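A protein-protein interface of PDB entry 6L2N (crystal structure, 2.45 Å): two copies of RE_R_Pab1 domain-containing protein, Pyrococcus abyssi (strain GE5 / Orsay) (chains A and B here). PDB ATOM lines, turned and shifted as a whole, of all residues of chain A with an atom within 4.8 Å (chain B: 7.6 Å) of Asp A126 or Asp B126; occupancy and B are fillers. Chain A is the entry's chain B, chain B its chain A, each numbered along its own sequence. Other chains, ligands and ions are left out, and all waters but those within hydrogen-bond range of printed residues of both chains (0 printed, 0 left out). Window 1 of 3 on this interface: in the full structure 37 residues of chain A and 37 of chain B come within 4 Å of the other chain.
Tyr A124 touches Pro B129. Tyr B128 touches Glu A125 (O to CA, 3.2 Å). O of Asp A126 touches CA of Val B127, at 3.1 Å. Asp A126 touches Val B130 (OD2 to CG1, 3.5 Å). CG1 of Val A127 touches CB of Glu B125, 3.5 Å away. Val A127 touches Asp B126. CG2 of Val A127 touches CG1 of Val B127, at 3.8 Å. Tyr A128 touches Tyr B124 (O to O, 3.8 Å). Tyr A128 touches Glu B125. OD1 of Asp B126 touches CG2 of Val A130, at 3.2 Å.
Printed residues of chain A that touch a printed residue of chain B: Arg A110, Arg A111, Tyr A124, Glu A125, Asp A126, Val A127, Tyr A128 and Val A130. Hydrophobic or aromatic side chains of chain A that line the printed part of chain B: Tyr A124, Val A127, Tyr A128 and Val A130. Along chain A the printed residues that touch a printed residue of chain B span positions 110 to 130. Among the printed residues, 21 pairs touch across the chains.
The guanidinium group (NH1) of Arg B110 lies within salt-bridge range of the side-chain carboxylate (OE2) of Glu B112 (3.0 Å). The backbone NH (N) of Val B127 lies within hydrogen-bond range of the backbone carbonyl oxygen (O) of Arg B110, at 3.0 Å. The guanidinium group (NE) of Arg B111 is in salt-bridge range of the side-chain carboxylate (OD2) of Asp B126, at 2.4 Å. The backbone NH of Glu B112 is in hydrogen-bond range of the backbone carbonyl oxygen of Glu B125. The backbone carbonyl oxygen of Val A127 sits at hydrogen-bond distance from the guanidinium group of Arg A110 (2.9 Å). The guanidinium group of Arg A111 lies within salt-bridge range of the side-chain carboxylate of Asp A126, at 2.7 Å.
Glu A125 touches Tyr B128, and with the chains exchanged Tyr A128 touches Glu B125. Val B127 touches its own counterpart, Val A127. Tyr A128 touches Tyr B124, but with the chains exchanged Tyr A124 does not touch Tyr B128 (4.1 Å). Tyr B128 touches its own counterpart, Tyr A128.
Asp A126 touches just these residues of chain B: Asp B126, Val B127, Tyr B128 and Val B130. Asp B126 touches four residues of chain A. Of the printed residues of chain B, Val A130 touches Arg B111, Tyr B124 and Asp B126. Of the printed residues of chain A, Arg B111 touches Val A130 (3.9 Å). Of the printed residues of chain B, Val A127 touches Glu B125, Asp B126 and Val B127. Leu B145 touches none of the printed residues of chain A. Ser B113 touches none of the printed residues of chain A. The nearest residue of chain B that does not touch Asp A126 is Pro B129 (5.0 Å). The nearest printed residue of chain A that does not touch Asp B126 is Arg A110 (6.8 Å). The nearest printed residue of chain B that does not touch Val A127 is Tyr B128 (4.9 Å).
OE1 of Glu A125 is in salt-bridge range of NH2 of Arg B110. N of Tyr B124 sits at hydrogen-bond distance from O of Val A130, 2.9 Å away. NH1 of Arg A110 is in salt-bridge range of OE2 of Glu B125, 3.7 Å away. The backbone carbonyl oxygen (O) of Asp B126 sits at hydrogen-bond distance from the backbone NH (N) of Tyr A128, 2.8 Å away. O of Asp A126 lies within hydrogen-bond range of N of Tyr B128, at 2.7 Å. The backbone carbonyl oxygen (O) of Val B130 sits at hydrogen-bond distance from the backbone NH (N) of Tyr A124 (2.8 Å). O of Asp B126 sits close to O of Asp A126 (3.4 Å).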
ATOM      1  N   ARG A 110      18.446  -6.543  17.007  1.00  0.00           N
ATOM      2  CA  ARG A 110      19.058  -5.320  16.513  1.00  0.00           C
ATOM      3  C   ARG A 110      20.180  -4.894  17.448  1.00  0.00           C
ATOM      4  O   ARG A 110      20.130  -5.142  18.655  1.00  0.00           O
ATOM      5  CB  ARG A 110      18.023  -4.198  16.380  1.00  0.00           C
ATOM      6  CG  ARG A 110      16.937  -4.470  15.348  1.00  0.00           C
ATOM      7  CD  ARG A 110      15.579  -4.571  16.023  1.00  0.00           C
ATOM      8  NE  ARG A 110      15.508  -5.707  16.940  1.00  0.00           N
ATOM      9  CZ  ARG A 110      14.709  -5.778  18.002  1.00  0.00           C
ATOM     10  NH1 ARG A 110      13.901  -4.775  18.313  1.00  0.00           N
ATOM     11  NH2 ARG A 110      14.718  -6.864  18.758  1.00  0.00           N
ATOM     12  N   ARG A 111      21.190  -4.243  16.879  1.00  0.00           N
ATOM     13  CA  ARG A 111      22.250  -3.601  17.654  1.00  0.00           C
ATOM     14  C   ARG A 111      22.115  -2.100  17.445  1.00  0.00           C
ATOM     15  O   ARG A 111      22.539  -1.567  16.418  1.00  0.00           O
ATOM     16  CB  ARG A 111      23.634  -4.103  17.259  1.00  0.00           C
ATOM     17  CG  ARG A 111      24.757  -3.284  17.907  1.00  0.00           C
ATOM     18  CD  ARG A 111      26.085  -4.020  17.883  1.00  0.00           C
ATOM     19  NE  ARG A 111      26.084  -5.191  18.756  1.00  0.00           N
ATOM     20  CZ  ARG A 111      27.053  -6.099  18.790  1.00  0.00           C
ATOM     21  NH1 ARG A 111      28.109  -5.981  17.995  1.00  0.00           N
ATOM     22  NH2 ARG A 111      26.967  -7.134  19.617  1.00  0.00           N
ATOM     23  N   TYR A 124      27.183   0.182  22.419  1.00  0.00           N
ATOM     24  CA  TYR A 124      25.963  -0.137  21.691  1.00  0.00           C
ATOM     25  C   TYR A 124      25.003  -0.867  22.626  1.00  0.00           C
ATOM     26  O   TYR A 124      25.314  -1.132  23.792  1.00  0.00           O
ATOM     27  CB  TYR A 124      26.252  -0.996  20.452  1.00  0.00           C
ATOM     28  CG  TYR A 124      27.288  -0.430  19.505  1.00  0.00           C
ATOM     29  CD1 TYR A 124      26.907   0.203  18.330  1.00  0.00           C
ATOM     30  CD2 TYR A 124      28.645  -0.549  19.777  1.00  0.00           C
ATOM     31  CE1 TYR A 124      27.846   0.717  17.458  1.00  0.00           C
ATOM     32  CE2 TYR A 124      29.591  -0.038  18.911  1.00  0.00           C
ATOM     33  CZ  TYR A 124      29.187   0.594  17.753  1.00  0.00           C
ATOM     34  OH  TYR A 124      30.125   1.104  16.886  1.00  0.00           O
ATOM     35  N   GLU A 125      23.826  -1.200  22.101  1.00  0.00           N
ATOM     36  CA  GLU A 125      22.842  -1.987  22.833  1.00  0.00           C
ATOM     37  C   GLU A 125      22.224  -3.012  21.895  1.00  0.00           C
ATOM     38  O   GLU A 125      21.785  -2.666  20.794  1.00  0.00           O
ATOM     39  CB  GLU A 125      21.743  -1.103  23.438  1.00  0.00           C
ATOM     40  CG  GLU A 125      22.224  -0.143  24.514  1.00  0.00           C
ATOM     41  CD  GLU A 125      21.081   0.513  25.264  1.00  0.00           C
ATOM     42  OE1 GLU A 125      21.111   0.512  26.512  1.00  0.00           O
ATOM     43  OE2 GLU A 125      20.153   1.026  24.606  1.00  0.00           O
ATOM     44  N   ASP A 126      22.196  -4.268  22.331  1.00  0.00           N
ATOM     45  CA  ASP A 126      21.487  -5.326  21.626  1.00  0.00           C
ATOM     46  C   ASP A 126      20.121  -5.516  22.265  1.00  0.00           C
ATOM     47  O   ASP A 126      20.025  -5.753  23.473  1.00  0.00           O
ATOM     48  CB  ASP A 126      22.266  -6.640  21.663  1.00  0.00           C
ATOM     49  CG  ASP A 126      23.643  -6.524  21.052  1.00  0.00           C
ATOM     50  OD1 ASP A 126      23.851  -5.619  20.215  1.00  0.00           O
ATOM     51  OD2 ASP A 126      24.515  -7.345  21.406  1.00  0.00           O
ATOM     52  N   VAL A 127      19.073  -5.415  21.456  1.00  0.00           N
ATOM     53  CA  VAL A 127      17.695  -5.564  21.915  1.00  0.00           C
ATOM     54  C   VAL A 127      17.175  -6.922  21.463  1.00  0.00           C
ATOM     55  O   VAL A 127      17.200  -7.235  20.266  1.00  0.00           O
ATOM     56  CB  VAL A 127      16.802  -4.429  21.382  1.00  0.00           C
ATOM     57  CG1 VAL A 127      15.390  -4.591  21.909  1.00  0.00           C
ATOM     58  CG2 VAL A 127      17.372  -3.073  21.777  1.00  0.00           C
ATOM     59  N   TYR A 128      16.692  -7.717  22.413  1.00  0.00           N
ATOM     60  CA  TYR A 128      16.152  -9.034  22.126  1.00  0.00           C
ATOM     61  C   TYR A 128      14.649  -9.038  22.344  1.00  0.00           C
ATOM     62  O   TYR A 128      14.183  -8.622  23.413  1.00  0.00           O
ATOM     63  CB  TYR A 128      16.810 -10.094  23.017  1.00  0.00           C
ATOM     64  CG  TYR A 128      18.254 -10.383  22.671  1.00  0.00           C
ATOM     65  CD1 TYR A 128      19.259  -9.479  22.992  1.00  0.00           C
ATOM     66  CD2 TYR A 128      18.612 -11.557  22.023  1.00  0.00           C
ATOM     67  CE1 TYR A 128      20.581  -9.737  22.676  1.00  0.00           C
ATOM     68  CE2 TYR A 128      19.931 -11.824  21.704  1.00  0.00           C
ATOM     69  CZ  TYR A 128      20.911 -10.910  22.034  1.00  0.00           C
ATOM     70  OH  TYR A 128      22.227 -11.168  21.719  1.00  0.00           O
ATOM     71  N   VAL A 130      11.015 -10.536  23.197  1.00  0.00           N
ATOM     72  CA  VAL A 130      10.466 -11.626  23.994  1.00  0.00           C
ATOM     73  C   VAL A 130       8.952 -11.488  24.016  1.00  0.00           C
ATOM     74  O   VAL A 130       8.428 -10.390  24.231  1.00  0.00           O
ATOM     75  CB  VAL A 130      11.031 -11.633  25.430  1.00  0.00           C
ATOM     76  CG1 VAL A 130      10.370 -12.724  26.261  1.00  0.00           C
ATOM     77  CG2 VAL A 130      12.542 -11.825  25.409  1.00  0.00           C
ATOM     78  N   ILE B 109      21.586  -4.764  32.586  1.00  0.00           N
ATOM     79  CA  ILE B 109      20.661  -5.424  31.672  1.00  0.00           C
ATOM     80  C   ILE B 109      19.247  -5.139  32.150  1.00  0.00           C
ATOM     81  O   ILE B 109      18.912  -5.413  33.309  1.00  0.00           O
ATOM     82  CB  ILE B 109      20.917  -6.941  31.595  1.00  0.00           C
ATOM     83  CG1 ILE B 109      22.364  -7.223  31.184  1.00  0.00           C
ATOM     84  CG2 ILE B 109      19.943  -7.598  30.626  1.00  0.00           C
ATOM     85  CD1 ILE B 109      22.799  -8.657  31.427  1.00  0.00           C
ATOM     86  N   ARG B 110      18.421  -4.587  31.266  1.00  0.00           N
ATOM     87  CA  ARG B 110      17.051  -4.231  31.601  1.00  0.00           C
ATOM     88  C   ARG B 110      16.079  -4.910  30.645  1.00  0.00           C
ATOM     89  O   ARG B 110      16.411  -5.196  29.490  1.00  0.00           O
ATOM     90  CB  ARG B 110      16.843  -2.703  31.566  1.00  0.00           C
ATOM     91  CG  ARG B 110      16.474  -2.140  30.199  1.00  0.00           C
ATOM     92  CD  ARG B 110      16.553  -0.616  30.167  1.00  0.00           C
ATOM     93  NE  ARG B 110      17.924  -0.144  29.982  1.00  0.00           N
ATOM     94  CZ  ARG B 110      18.380   0.436  28.875  1.00  0.00           C
ATOM     95  NH1 ARG B 110      17.576   0.619  27.837  1.00  0.00           N
ATOM     96  NH2 ARG B 110      19.646   0.824  28.805  1.00  0.00           N
ATOM     97  N   ARG B 111      14.877  -5.180  31.146  1.00  0.00           N
ATOM     98  CA  ARG B 111      13.765  -5.649  30.328  1.00  0.00           C
ATOM     99  C   ARG B 111      12.790  -4.489  30.174  1.00  0.00           C
ATOM    100  O   ARG B 111      12.147  -4.077  31.143  1.00  0.00           O
ATOM    101  CB  ARG B 111      13.081  -6.866  30.948  1.00  0.00           C
ATOM    102  CG  ARG B 111      11.637  -7.065  30.483  1.00  0.00           C
ATOM    103  CD  ARG B 111      11.201  -8.517  30.599  1.00  0.00           C
ATOM    104  NE  ARG B 111      12.147  -9.432  29.964  1.00  0.00           N
ATOM    105  CZ  ARG B 111      11.986 -10.751  29.914  1.00  0.00           C
ATOM    106  NH1 ARG B 111      10.915 -11.303  30.465  1.00  0.00           N
ATOM    107  NH2 ARG B 111      12.894 -11.517  29.320  1.00  0.00           N
ATOM    108  N   GLU B 112      12.691  -3.954  28.963  1.00  0.00           N
ATOM    109  CA  GLU B 112      11.819  -2.821  28.700  1.00  0.00           C
ATOM    110  C   GLU B 112      10.422  -3.303  28.336  1.00  0.00           C
ATOM    111  O   GLU B 112      10.259  -4.265  27.581  1.00  0.00           O
ATOM    112  CB  GLU B 112      12.380  -1.962  27.567  1.00  0.00           C
ATOM    113  CG  GLU B 112      13.755  -1.389  27.838  1.00  0.00           C
ATOM    114  CD  GLU B 112      13.726   0.101  28.092  1.00  0.00           C
ATOM    115  OE1 GLU B 112      12.803   0.572  28.792  1.00  0.00           O
ATOM    116  OE2 GLU B 112      14.627   0.803  27.584  1.00  0.00           O
ATOM    117  N   SER B 113       9.415  -2.632  28.885  1.00  0.00           N
ATOM    118  CA  SER B 113       8.048  -2.843  28.438  1.00  0.00           C
ATOM    119  C   SER B 113       7.808  -2.065  27.150  1.00  0.00           C
ATOM    120  O   SER B 113       8.447  -1.042  26.886  1.00  0.00           O
ATOM    121  CB  SER B 113       7.047  -2.414  29.513  1.00  0.00           C
ATOM    122  OG  SER B 113       7.322  -1.106  29.987  1.00  0.00           O
ATOM    123  N   THR B 114       6.882  -2.568  26.338  1.00  0.00           N
ATOM    124  CA  THR B 114       6.593  -1.987  25.038  1.00  0.00           C
ATOM    125  C   THR B 114       5.108  -1.675  24.926  1.00  0.00           C
ATOM    126  O   THR B 114       4.274  -2.230  25.645  1.00  0.00           O
ATOM    127  CB  THR B 114       6.998  -2.924  23.889  1.00  0.00           C
ATOM    128  OG1 THR B 114       6.031  -3.975  23.767  1.00  0.00           O
ATOM    129  CG2 THR B 114       8.376  -3.531  24.138  1.00  0.00           C
ATOM    130  N   TYR B 124       8.092  -7.703  25.271  1.00  0.00           N
ATOM    131  CA  TYR B 124       9.149  -7.053  26.028  1.00  0.00           C
ATOM    132  C   TYR B 124      10.408  -6.954  25.177  1.00  0.00           C
ATOM    133  O   TYR B 124      10.583  -7.684  24.197  1.00  0.00           O
ATOM    134  CB  TYR B 124       9.472  -7.817  27.318  1.00  0.00           C
ATOM    135  CG  TYR B 124       8.413  -7.750  28.391  1.00  0.00           C
ATOM    136  CD1 TYR B 124       8.050  -6.538  28.967  1.00  0.00           C
ATOM    137  CD2 TYR B 124       7.796  -8.905  28.851  1.00  0.00           C
ATOM    138  CE1 TYR B 124       7.091  -6.480  29.959  1.00  0.00           C
ATOM    139  CE2 TYR B 124       6.837  -8.857  29.841  1.00  0.00           C
ATOM    140  CZ  TYR B 124       6.489  -7.643  30.391  1.00  0.00           C
ATOM    141  OH  TYR B 124       5.535  -7.597  31.380  1.00  0.00           O
ATOM    142  N   GLU B 125      11.297  -6.048  25.573  1.00  0.00           N
ATOM    143  CA  GLU B 125      12.583  -5.867  24.909  1.00  0.00           C
ATOM    144  C   GLU B 125      13.679  -5.886  25.966  1.00  0.00           C
ATOM    145  O   GLU B 125      13.795  -4.948  26.761  1.00  0.00           O
ATOM    146  CB  GLU B 125      12.616  -4.564  24.108  1.00  0.00           C
ATOM    147  CG  GLU B 125      11.801  -4.597  22.821  1.00  0.00           C
ATOM    148  CD  GLU B 125      11.842  -3.278  22.069  1.00  0.00           C
ATOM    149  OE1 GLU B 125      12.019  -2.227  22.720  1.00  0.00           O
ATOM    150  OE2 GLU B 125      11.697  -3.292  20.828  1.00  0.00           O
ATOM    151  N   ASP B 126      14.473  -6.955  25.983  1.00  0.00           N
ATOM    152  CA  ASP B 126      15.637  -7.044  26.855  1.00  0.00           C
ATOM    153  C   ASP B 126      16.837  -6.460  26.121  1.00  0.00           C
ATOM    154  O   ASP B 126      17.247  -6.986  25.081  1.00  0.00           O
ATOM    155  CB  ASP B 126      15.914  -8.490  27.265  1.00  0.00           C
ATOM    156  CG  ASP B 126      14.682  -9.199  27.786  1.00  0.00           C
ATOM    157  OD1 ASP B 126      14.519 -10.402  27.499  1.00  0.00           O
ATOM    158  OD2 ASP B 126      13.873  -8.556  28.482  1.00  0.00           O
ATOM    159  N   VAL B 127      17.396  -5.377  26.652  1.00  0.00           N
ATOM    160  CA  VAL B 127      18.522  -4.697  26.025  1.00  0.00           C
ATOM    161  C   VAL B 127      19.792  -5.053  26.790  1.00  0.00           C
ATOM    162  O   VAL B 127      19.799  -5.094  28.027  1.00  0.00           O
ATOM    163  CB  VAL B 127      18.293  -3.175  25.944  1.00  0.00           C
ATOM    164  CG1 VAL B 127      16.855  -2.882  25.515  1.00  0.00           C
ATOM    165  CG2 VAL B 127      18.603  -2.489  27.257  1.00  0.00           C
ATOM    166  N   TYR B 128      20.856  -5.357  26.045  1.00  0.00           N
ATOM    167  CA  TYR B 128      22.147  -5.759  26.580  1.00  0.00           C
ATOM    168  C   TYR B 128      23.230  -4.807  26.086  1.00  0.00           C
ATOM    169  O   TYR B 128      23.238  -4.440  24.906  1.00  0.00           O
ATOM    170  CB  TYR B 128      22.504  -7.197  26.165  1.00  0.00           C
ATOM    171  CG  TYR B 128      21.621  -8.270  26.775  1.00  0.00           C
ATOM    172  CD1 TYR B 128      20.310  -8.443  26.348  1.00  0.00           C
ATOM    173  CD2 TYR B 128      22.102  -9.115  27.769  1.00  0.00           C
ATOM    174  CE1 TYR B 128      19.500  -9.419  26.897  1.00  0.00           C
ATOM    175  CE2 TYR B 128      21.297 -10.097  28.325  1.00  0.00           C
ATOM    176  CZ  TYR B 128      19.995 -10.242  27.884  1.00  0.00           C
ATOM    177  OH  TYR B 128      19.183 -11.212  28.425  1.00  0.00           O
ATOM    178  N   PRO B 129      24.149  -4.386  26.954  1.00  0.00           N
ATOM    179  CA  PRO B 129      25.198  -3.456  26.525  1.00  0.00           C
ATOM    180  C   PRO B 129      26.402  -4.179  25.941  1.00  0.00           C
ATOM    181  O   PRO B 129      26.803  -5.252  26.397  1.00  0.00           O
ATOM    182  CB  PRO B 129      25.561  -2.740  27.831  1.00  0.00           C
ATOM    183  CG  PRO B 129      25.377  -3.799  28.872  1.00  0.00           C
ATOM    184  CD  PRO B 129      24.238  -4.686  28.395  1.00  0.00           C
ATOM    185  N   VAL B 130      26.976  -3.577  24.903  1.00  0.00           N
ATOM    186  CA  VAL B 130      28.174  -4.100  24.255  1.00  0.00           C
ATOM    187  C   VAL B 130      29.130  -2.944  23.995  1.00  0.00           C
ATOM    188  O   VAL B 130      28.705  -1.843  23.629  1.00  0.00           O
ATOM    189  CB  VAL B 130      27.846  -4.846  22.942  1.00  0.00           C
ATOM    190  CG1 VAL B 130      27.344  -6.252  23.238  1.00  0.00           C
ATOM    191  CG2 VAL B 130      26.818  -4.078  22.133  1.00  0.00           C
ATOM    192  N   VAL B 144      30.936  -7.816  25.980  1.00  0.00           N
ATOM    193  CA  VAL B 144      29.507  -8.046  26.142  1.00  0.00           C
ATOM    194  C   VAL B 144      29.229  -8.326  27.612  1.00  0.00           C
ATOM    195  O   VAL B 144      30.064  -8.909  28.316  1.00  0.00           O
ATOM    196  CB  VAL B 144      28.999  -9.193  25.243  1.00  0.00           C
ATOM    197  CG1 VAL B 144      29.596  -9.083  23.848  1.00  0.00           C
ATOM    198  CG2 VAL B 144      29.309 -10.549  25.851  1.00  0.00           C
ATOM    199  N   LEU B 145      28.069  -7.879  28.079  1.00  0.00           N
ATOM    200  CA  LEU B 145      27.617  -8.119  29.440  1.00  0.00           C
ATOM    201  C   LEU B 145      26.544  -9.197  29.429  1.00  0.00           C
ATOM    202  O   LEU B 145      25.744  -9.280  28.491  1.00  0.00           O
ATOM    203  CB  LEU B 145      27.065  -6.838  30.072  1.00  0.00           C
ATOM    204  CG  LEU B 145      26.976  -6.810  31.600  1.00  0.00           C
ATOM    205  CD1 LEU B 145      28.362  -6.892  32.208  1.00  0.00           C
ATOM    206  CD2 LEU B 145      26.241  -5.565  32.090  1.00  0.00           C
ATOM    207  N   HIS B 147      24.105 -11.930  32.331  1.00  0.00           N
ATOM    208  CA  HIS B 147      23.753 -12.309  33.692  1.00  0.00           C
ATOM    209  C   HIS B 147      24.672 -13.420  34.182  1.00  0.00           C
ATOM    210  O   HIS B 147      24.930 -14.390  33.462  1.00  0.00           O
ATOM    211  CB  HIS B 147      22.298 -12.772  33.752  1.00  0.00           C
ATOM    212  CG  HIS B 147      21.317 -11.664  33.979  1.00  0.00           C
ATOM    213  ND1 HIS B 147      20.455 -11.222  32.998  1.00  0.00           N
ATOM    214  CD2 HIS B 147      21.053 -10.917  35.077  1.00  0.00           C
ATOM    215  CE1 HIS B 147      19.705 -10.247  33.482  1.00  0.00           C
ATOM    216  NE2 HIS B 147      20.049 -10.043  34.741  1.00  0.00           N
